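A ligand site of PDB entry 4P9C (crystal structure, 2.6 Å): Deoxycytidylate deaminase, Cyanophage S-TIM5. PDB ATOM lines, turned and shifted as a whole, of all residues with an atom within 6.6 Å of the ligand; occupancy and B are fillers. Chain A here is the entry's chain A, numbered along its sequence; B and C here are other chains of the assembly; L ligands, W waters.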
ATOM      1  N   PHE A  19     -24.351  -0.289  -4.086  1.00  0.00           N
ATOM      2  CA  PHE A  19     -24.525  -1.097  -5.299  1.00  0.00           C
ATOM      3  C   PHE A  19     -25.991  -1.258  -5.724  1.00  0.00           C
ATOM      4  O   PHE A  19     -26.268  -1.572  -6.886  1.00  0.00           O
ATOM      5  CB  PHE A  19     -23.860  -2.466  -5.153  1.00  0.00           C
ATOM      6  CG  PHE A  19     -22.384  -2.427  -5.378  1.00  0.00           C
ATOM      7  CD1 PHE A  19     -21.855  -2.488  -6.665  1.00  0.00           C
ATOM      8  CD2 PHE A  19     -21.511  -2.308  -4.300  1.00  0.00           C
ATOM      9  CE1 PHE A  19     -20.483  -2.436  -6.873  1.00  0.00           C
ATOM     10  CE2 PHE A  19     -20.139  -2.261  -4.496  1.00  0.00           C
ATOM     11  CZ  PHE A  19     -19.618  -2.329  -5.791  1.00  0.00           C
ATOM     12  N   HIS A  43     -20.860  -8.720  -5.573  1.00  0.00           N
ATOM     13  CA  HIS A  43     -21.833  -7.658  -5.413  1.00  0.00           C
ATOM     14  C   HIS A  43     -22.897  -7.711  -6.489  1.00  0.00           C
ATOM     15  O   HIS A  43     -22.649  -7.485  -7.622  1.00  0.00           O
ATOM     16  CB  HIS A  43     -21.181  -6.296  -5.380  1.00  0.00           C
ATOM     17  CG  HIS A  43     -20.287  -6.007  -6.532  1.00  0.00           C
ATOM     18  ND1 HIS A  43     -18.946  -5.827  -6.379  1.00  0.00           N
ATOM     19  CD2 HIS A  43     -20.532  -5.849  -7.837  1.00  0.00           C
ATOM     20  CE1 HIS A  43     -18.397  -5.578  -7.549  1.00  0.00           C
ATOM     21  NE2 HIS A  43     -19.351  -5.592  -8.452  1.00  0.00           N
ATOM     22  N   GLY A  44     -24.110  -8.038  -6.092  1.00  0.00           N
ATOM     23  CA  GLY A  44     -25.232  -8.214  -6.998  1.00  0.00           C
ATOM     24  C   GLY A  44     -26.320  -7.192  -6.786  1.00  0.00           C
ATOM     25  O   GLY A  44     -26.591  -6.781  -5.653  1.00  0.00           O
ATOM     26  N   TRP A  45     -26.954  -6.790  -7.881  1.00  0.00           N
ATOM     27  CA  TRP A  45     -28.116  -5.928  -7.820  1.00  0.00           C
ATOM     28  C   TRP A  45     -29.148  -6.408  -8.822  1.00  0.00           C
ATOM     29  O   TRP A  45     -28.806  -7.091  -9.792  1.00  0.00           O
ATOM     30  CB  TRP A  45     -27.732  -4.467  -8.092  1.00  0.00           C
ATOM     31  CG  TRP A  45     -27.137  -4.270  -9.448  1.00  0.00           C
ATOM     32  CD1 TRP A  45     -27.820  -4.102 -10.615  1.00  0.00           C
ATOM     33  CD2 TRP A  45     -25.750  -4.222  -9.779  1.00  0.00           C
ATOM     34  NE1 TRP A  45     -26.940  -3.946 -11.655  1.00  0.00           N
ATOM     35  CE2 TRP A  45     -25.660  -4.015 -11.181  1.00  0.00           C
ATOM     36  CE3 TRP A  45     -24.571  -4.332  -9.036  1.00  0.00           C
ATOM     37  CZ2 TRP A  45     -24.443  -3.919 -11.846  1.00  0.00           C
ATOM     38  CZ3 TRP A  45     -23.346  -4.235  -9.709  1.00  0.00           C
ATOM     39  CH2 TRP A  45     -23.298  -4.027 -11.094  1.00  0.00           C
ATOM     40  N   ASN A  46     -30.417  -6.056  -8.597  1.00  0.00           N
ATOM     41  CA  ASN A  46     -31.500  -6.484  -9.473  1.00  0.00           C
ATOM     42  C   ASN A  46     -31.446  -5.839 -10.855  1.00  0.00           C
ATOM     43  O   ASN A  46     -31.166  -4.645 -10.982  1.00  0.00           O
ATOM     44  CB  ASN A  46     -32.887  -6.297  -8.827  1.00  0.00           C
ATOM     45  CG  ASN A  46     -33.134  -4.869  -8.328  1.00  0.00           C
ATOM     46  OD1 ASN A  46     -32.211  -4.132  -7.988  1.00  0.00           O
ATOM     47  ND2 ASN A  46     -34.409  -4.492  -8.267  1.00  0.00           N
ATOM     48  N   GLY A  47     -31.689  -6.653 -11.887  1.00  0.00           N
ATOM     49  CA  GLY A  47     -31.673  -6.174 -13.265  1.00  0.00           C
ATOM     50  C   GLY A  47     -31.940  -7.271 -14.274  1.00  0.00           C
ATOM     51  O   GLY A  47     -32.010  -8.449 -13.927  1.00  0.00           O
ATOM     52  N   THR A  48     -32.102  -6.866 -15.527  1.00  0.00           N
ATOM     53  CA  THR A  48     -32.205  -7.809 -16.633  1.00  0.00           C
ATOM     54  C   THR A  48     -30.846  -8.477 -16.862  1.00  0.00           C
ATOM     55  O   THR A  48     -29.816  -7.922 -16.486  1.00  0.00           O
ATOM     56  CB  THR A  48     -32.662  -7.121 -17.937  1.00  0.00           C
ATOM     57  OG1 THR A  48     -31.752  -6.055 -18.268  1.00  0.00           O
ATOM     58  CG2 THR A  48     -34.066  -6.555 -17.795  1.00  0.00           C
ATOM     59  N   PRO A  49     -30.837  -9.682 -17.480  1.00  0.00           N
ATOM     60  CA  PRO A  49     -29.599 -10.408 -17.760  1.00  0.00           C
ATOM     61  C   PRO A  49     -28.652  -9.655 -18.699  1.00  0.00           C
ATOM     62  O   PRO A  49     -29.090  -8.783 -19.451  1.00  0.00           O
ATOM     63  CB  PRO A  49     -30.081 -11.681 -18.453  1.00  0.00           C
ATOM     64  CG  PRO A  49     -31.487 -11.844 -17.997  1.00  0.00           C
ATOM     65  CD  PRO A  49     -32.016 -10.460 -17.882  1.00  0.00           C
ATOM     66  N   SER A  50     -27.366  -9.992 -18.635  1.00  0.00           N
ATOM     67  CA  SER A  50     -26.349  -9.333 -19.460  1.00  0.00           C
ATOM     68  C   SER A  50     -26.627  -9.523 -20.953  1.00  0.00           C
ATOM     69  O   SER A  50     -26.780 -10.650 -21.431  1.00  0.00           O
ATOM     70  CB  SER A  50     -24.953  -9.847 -19.125  1.00  0.00           C
ATOM     71  OG  SER A  50     -24.559  -9.419 -17.824  1.00  0.00           O
ATOM     72  N   GLY A  51     -26.716  -8.398 -21.656  1.00  0.00           N
ATOM     73  CA  GLY A  51     -26.962  -8.396 -23.099  1.00  0.00           C
ATOM     74  C   GLY A  51     -28.417  -8.547 -23.499  1.00  0.00           C
ATOM     75  O   GLY A  51     -28.709  -8.873 -24.649  1.00  0.00           O
ATOM     76  N   ASN A  55     -32.871  -2.443 -20.627  1.00  0.00           N
ATOM     77  CA  ASN A  55     -32.507  -2.231 -19.243  1.00  0.00           C
ATOM     78  C   ASN A  55     -33.674  -2.252 -18.261  1.00  0.00           C
ATOM     79  O   ASN A  55     -33.492  -2.574 -17.071  1.00  0.00           O
ATOM     80  CB  ASN A  55     -31.812  -0.891 -19.107  1.00  0.00           C
ATOM     81  CG  ASN A  55     -30.320  -0.982 -19.275  1.00  0.00           C
ATOM     82  OD1 ASN A  55     -29.750  -2.068 -19.340  1.00  0.00           O
ATOM     83  ND2 ASN A  55     -29.666   0.170 -19.346  1.00  0.00           N
ATOM     84  N   VAL A  68     -35.843 -10.651 -15.265  1.00  0.00           N
ATOM     85  CA  VAL A  68     -34.913  -9.960 -14.356  1.00  0.00           C
ATOM     86  C   VAL A  68     -34.405 -10.863 -13.236  1.00  0.00           C
ATOM     87  O   VAL A  68     -35.140 -11.728 -12.737  1.00  0.00           O
ATOM     88  CB  VAL A  68     -35.489  -8.649 -13.754  1.00  0.00           C
ATOM     89  CG1 VAL A  68     -36.098  -7.783 -14.837  1.00  0.00           C
ATOM     90  CG2 VAL A  68     -36.489  -8.946 -12.645  1.00  0.00           C
ATOM     91  N   LEU A  69     -33.159 -10.645 -12.862  1.00  0.00           N
ATOM     92  CA  LEU A  69     -32.526 -11.428 -11.811  1.00  0.00           C
ATOM     93  C   LEU A  69     -32.576 -10.645 -10.505  1.00  0.00           C
ATOM     94  O   LEU A  69     -32.323  -9.440 -10.493  1.00  0.00           O
ATOM     95  CB  LEU A  69     -31.092 -11.767 -12.197  1.00  0.00           C
ATOM     96  CG  LEU A  69     -30.945 -12.800 -13.325  1.00  0.00           C
ATOM     97  CD1 LEU A  69     -29.966 -12.330 -14.395  1.00  0.00           C
ATOM     98  CD2 LEU A  69     -30.538 -14.160 -12.758  1.00  0.00           C
ATOM     99  N   HIS A  70     -32.924 -11.328  -9.422  1.00  0.00           N
ATOM    100  CA  HIS A  70     -32.892 -10.739  -8.092  1.00  0.00           C
ATOM    101  C   HIS A  70     -31.437 -10.493  -7.688  1.00  0.00           C
ATOM    102  O   HIS A  70     -30.529 -11.156  -8.199  1.00  0.00           O
ATOM    103  CB  HIS A  70     -33.592 -11.662  -7.097  1.00  0.00           C
ATOM    104  CG  HIS A  70     -35.090 -11.667  -7.211  1.00  0.00           C
ATOM    105  ND1 HIS A  70     -35.915 -11.959  -6.147  1.00  0.00           N
ATOM    106  CD2 HIS A  70     -35.902 -11.429  -8.265  1.00  0.00           C
ATOM    107  CE1 HIS A  70     -37.181 -11.898  -6.542  1.00  0.00           C
ATOM    108  NE2 HIS A  70     -37.192 -11.575  -7.823  1.00  0.00           N
ATOM    109  N   ALA A  71     -31.224  -9.545  -6.781  1.00  0.00           N
ATOM    110  CA  ALA A  71     -29.876  -9.238  -6.313  1.00  0.00           C
ATOM    111  C   ALA A  71     -29.191 -10.471  -5.730  1.00  0.00           C
ATOM    112  O   ALA A  71     -27.981 -10.663  -5.926  1.00  0.00           O
ATOM    113  CB  ALA A  71     -29.912  -8.115  -5.286  1.00  0.00           C
ATOM    114  N   ASN A  74     -28.159 -12.798  -8.551  1.00  0.00           N
ATOM    115  CA  ASN A  74     -26.967 -12.279  -9.216  1.00  0.00           C
ATOM    116  C   ASN A  74     -25.697 -12.502  -8.413  1.00  0.00           C
ATOM    117  O   ASN A  74     -24.648 -12.774  -9.012  1.00  0.00           O
ATOM    118  CB  ASN A  74     -27.145 -10.796  -9.542  1.00  0.00           C
ATOM    119  CG  ASN A  74     -27.849 -10.575 -10.854  1.00  0.00           C
ATOM    120  OD1 ASN A  74     -27.641 -11.301 -11.817  1.00  0.00           O
ATOM    121  ND2 ASN A  74     -28.697  -9.550 -10.902  1.00  0.00           N
ATOM    122  N   ALA A  75     -25.792 -12.390  -7.094  1.00  0.00           N
ATOM    123  CA  ALA A  75     -24.651 -12.656  -6.224  1.00  0.00           C
ATOM    124  C   ALA A  75     -24.317 -14.136  -6.206  1.00  0.00           C
ATOM    125  O   ALA A  75     -23.140 -14.520  -6.167  1.00  0.00           O
ATOM    126  CB  ALA A  75     -24.924 -12.146  -4.815  1.00  0.00           C
ATOM    127  N   LYS A  78     -22.770 -14.998  -9.505  1.00  0.00           N
ATOM    128  CA  LYS A  78     -21.454 -14.392  -9.486  1.00  0.00           C
ATOM    129  C   LYS A  78     -20.461 -15.291  -8.756  1.00  0.00           C
ATOM    130  O   LYS A  78     -19.308 -15.420  -9.167  1.00  0.00           O
ATOM    131  CB  LYS A  78     -21.519 -13.045  -8.784  1.00  0.00           C
ATOM    132  CG  LYS A  78     -20.417 -12.066  -9.149  1.00  0.00           C
ATOM    133  CD  LYS A  78     -20.719 -11.350 -10.458  1.00  0.00           C
ATOM    134  CE  LYS A  78     -19.776 -10.180 -10.672  1.00  0.00           C
ATOM    135  NZ  LYS A  78     -19.998  -9.076  -9.680  1.00  0.00           N
ATOM    136  N   GLN B 107     -27.026 -16.539 -17.252  1.00  0.00           N
ATOM    137  CA  GLN B 107     -26.270 -15.483 -16.597  1.00  0.00           C
ATOM    138  C   GLN B 107     -24.941 -16.013 -16.055  1.00  0.00           C
ATOM    139  O   GLN B 107     -23.957 -15.278 -15.959  1.00  0.00           O
ATOM    140  CB  GLN B 107     -27.105 -14.838 -15.480  1.00  0.00           C
ATOM    141  CG  GLN B 107     -26.459 -13.644 -14.763  1.00  0.00           C
ATOM    142  CD  GLN B 107     -26.476 -12.345 -15.574  1.00  0.00           C
ATOM    143  OE1 GLN B 107     -27.216 -12.210 -16.555  1.00  0.00           O
ATOM    144  NE2 GLN B 107     -25.644 -11.389 -15.168  1.00  0.00           N
ATOM    145  N   LYS C   5     -19.146   1.988 -16.799  1.00  0.00           N
ATOM    146  CA  LYS C   5     -20.218   2.959 -16.636  1.00  0.00           C
ATOM    147  C   LYS C   5     -19.967   3.849 -15.421  1.00  0.00           C
ATOM    148  O   LYS C   5     -19.532   3.348 -14.373  1.00  0.00           O
ATOM    149  CB  LYS C   5     -21.581   2.248 -16.540  1.00  0.00           C
ATOM    150  CG  LYS C   5     -22.052   1.647 -17.860  1.00  0.00           C
ATOM    151  CD  LYS C   5     -23.361   0.872 -17.699  1.00  0.00           C
ATOM    152  CE  LYS C   5     -23.144  -0.540 -17.163  1.00  0.00           C
ATOM    153  NZ  LYS C   5     -22.396  -1.405 -18.127  1.00  0.00           N
ATOM    154  N   ILE C   8     -21.064   2.819 -11.871  1.00  0.00           N
ATOM    155  CA  ILE C   8     -20.207   1.781 -11.288  1.00  0.00           C
ATOM    156  C   ILE C   8     -18.886   2.368 -10.781  1.00  0.00           C
ATOM    157  O   ILE C   8     -18.430   2.029  -9.685  1.00  0.00           O
ATOM    158  CB  ILE C   8     -19.974   0.620 -12.308  1.00  0.00           C
ATOM    159  CG1 ILE C   8     -21.097  -0.431 -12.193  1.00  0.00           C
ATOM    160  CG2 ILE C   8     -18.595  -0.034 -12.150  1.00  0.00           C
ATOM    161  CD1 ILE C   8     -21.140  -1.210 -10.866  1.00  0.00           C
ATOM    162  N   TYR C  12     -17.617   2.352  -6.791  1.00  0.00           N
ATOM    163  CA  TYR C  12     -16.339   1.891  -6.267  1.00  0.00           C
ATOM    164  C   TYR C  12     -15.615   2.965  -5.461  1.00  0.00           C
ATOM    165  O   TYR C  12     -15.022   2.666  -4.426  1.00  0.00           O
ATOM    166  CB  TYR C  12     -15.436   1.362  -7.384  1.00  0.00           C
ATOM    167  CG  TYR C  12     -15.873   0.031  -7.965  1.00  0.00           C
ATOM    168  CD1 TYR C  12     -16.141  -1.061  -7.142  1.00  0.00           C
ATOM    169  CD2 TYR C  12     -15.979  -0.144  -9.341  1.00  0.00           C
ATOM    170  CE1 TYR C  12     -16.529  -2.289  -7.673  1.00  0.00           C
ATOM    171  CE2 TYR C  12     -16.361  -1.370  -9.880  1.00  0.00           C
ATOM    172  CZ  TYR C  12     -16.632  -2.445  -9.043  1.00  0.00           C
ATOM    173  OH  TYR C  12     -17.017  -3.654  -9.569  1.00  0.00           O
ATOM    174  N   ASN C  37     -12.743  -7.450 -12.888  1.00  0.00           N
ATOM    175  CA  ASN C  37     -13.906  -8.135 -13.476  1.00  0.00           C
ATOM    176  C   ASN C  37     -15.169  -8.029 -12.625  1.00  0.00           C
ATOM    177  O   ASN C  37     -15.937  -9.002 -12.515  1.00  0.00           O
ATOM    178  CB  ASN C  37     -13.586  -9.608 -13.754  1.00  0.00           C
ATOM    179  CG  ASN C  37     -12.376  -9.794 -14.654  1.00  0.00           C
ATOM    180  OD1 ASN C  37     -12.354  -9.341 -15.801  1.00  0.00           O
ATOM    181  ND2 ASN C  37     -11.357 -10.466 -14.131  1.00  0.00           N
ATOM    182  N   GLY C  38     -15.399  -6.850 -12.034  1.00  0.00           N
ATOM    183  CA  GLY C  38     -16.543  -6.642 -11.138  1.00  0.00           C
ATOM    184  C   GLY C  38     -16.431  -7.429  -9.837  1.00  0.00           C
ATOM    185  O   GLY C  38     -17.342  -8.173  -9.474  1.00  0.00           O
ATOM    186  N   SER C  39     -15.303  -7.257  -9.143  1.00  0.00           N
ATOM    187  CA  SER C  39     -15.085  -7.902  -7.842  1.00  0.00           C
ATOM    188  C   SER C  39     -14.127  -7.096  -6.970  1.00  0.00           C
ATOM    189  O   SER C  39     -13.016  -6.764  -7.389  1.00  0.00           O
ATOM    190  CB  SER C  39     -14.563  -9.331  -8.040  1.00  0.00           C
ATOM    191  OG  SER C  39     -14.563 -10.041  -6.812  1.00  0.00           O
HETATM  192  N1  LIG L   1     -24.572  -7.653 -12.424  1.00  0.00           N
HETATM  193  C1  LIG L   1     -24.288  -7.705 -11.106  1.00  0.00           C
HETATM  194  N2  LIG L   1     -23.010  -7.329 -10.648  1.00  0.00           N
HETATM  195  C2  LIG L   1     -22.036  -6.899 -11.566  1.00  0.00           C
HETATM  196  C3  LIG L   1     -22.330  -6.844 -12.920  1.00  0.00           C
HETATM  197  C4  LIG L   1     -23.599  -7.233 -13.346  1.00  0.00           C
HETATM  198  O1  LIG L   1     -25.127  -8.072 -10.285  1.00  0.00           O
HETATM  199  N3  LIG L   1     -20.841  -6.532 -11.130  1.00  0.00           N
HETATM  200  C5  LIG L   1     -25.916  -8.068 -12.922  1.00  0.00           C
HETATM  201  C6  LIG L   1     -26.970  -6.994 -12.724  1.00  0.00           C
HETATM  202  C7  LIG L   1     -27.836  -7.118 -13.947  1.00  0.00           C
HETATM  203  C8  LIG L   1     -26.879  -7.592 -15.032  1.00  0.00           C
HETATM  204  O2  LIG L   1     -25.835  -8.344 -14.351  1.00  0.00           O
HETATM  205  O3  LIG L   1     -28.837  -8.139 -13.730  1.00  0.00           O
HETATM  206  C9  LIG L   1     -26.308  -6.384 -15.792  1.00  0.00           C
HETATM  207  O4  LIG L   1     -25.481  -6.873 -16.861  1.00  0.00           O
HETATM  208  P1  LIG L   1     -24.309  -5.950 -17.444  1.00  0.00           P
HETATM  209  O5  LIG L   1     -23.333  -5.521 -16.419  1.00  0.00           O
HETATM  210  O6  LIG L   1     -23.617  -6.788 -18.643  1.00  0.00           O
HETATM  211  O7  LIG L   1     -25.034  -4.694 -18.166  1.00  0.00           O
HETATM  212  O   HOH W   1     -22.422  -3.222 -15.155  1.00  0.00           O
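The side-chain hydroxyl of Ser 50 is in hydrogen-bond range of an oxygen (O4) of the ligand, 2.9 Å away.
O of Thr 48 sits at hydrogen-bond distance from O3 of the ligand (2.9 Å).
NE2 of His 43 sits at hydrogen-bond distance from N3 of the ligand (3.2 Å).
An oxygen (O2) of the ligand lies within hydrogen-bond range of the side-chain amide nitrogen of Gln 107 of chain B, at 3.2 Å.
An oxygen (O3) of the ligand sits at hydrogen-bond distance from the side-chain amide nitrogen (ND2) of Asn 74 (3.2 Å).
N of Trp 45 sits at hydrogen-bond distance from O1 of the ligand (3.3 Å).
The backbone carbonyl oxygen (O) of Gly 47 is in hydrogen-bond range of an oxygen (O3) of the ligand, at 3.2 Å.
The side-chain amide oxygen of Gln 107 of chain B lies within hydrogen-bond range of the backbone NH of Ser 50 (3.0 Å).
O of Gly 38 of chain C lies within hydrogen-bond range of NZ of Lys 78 (2.8 Å).
O of Gly 38 of chain C lies close to NE2 of His 43 (3.4 Å).
The side-chain hydroxyl (OH) of Tyr 12 of chain C lies close to a ring nitrogen (NE2) of His 43, at 3.2 Å.
ND2 of Asn 74 sits at hydrogen-bond distance from O of Trp 45.
O of Gly 47 is in hydrogen-bond range of N of Leu 69 (2.7 Å).
N3 of the ligand lies close to NZ of Lys 78 (3.0 Å).
CA of Gly 44 touches O1 of the ligand, at 3.3 Å.
Hydrophobic or aromatic side chains that line the ligand: His 43 and Trp 45.
Within 4 Å of the ligand: His 43, Gly 44, Trp 45, Gly 47, Thr 48, Ser 50, Asn 74, Lys 78 and Gln 107 of chain B.
Water W1 bridges O5 of the ligand (2.8 Å) and NZ of Lys 5 of chain C (3.5 Å).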
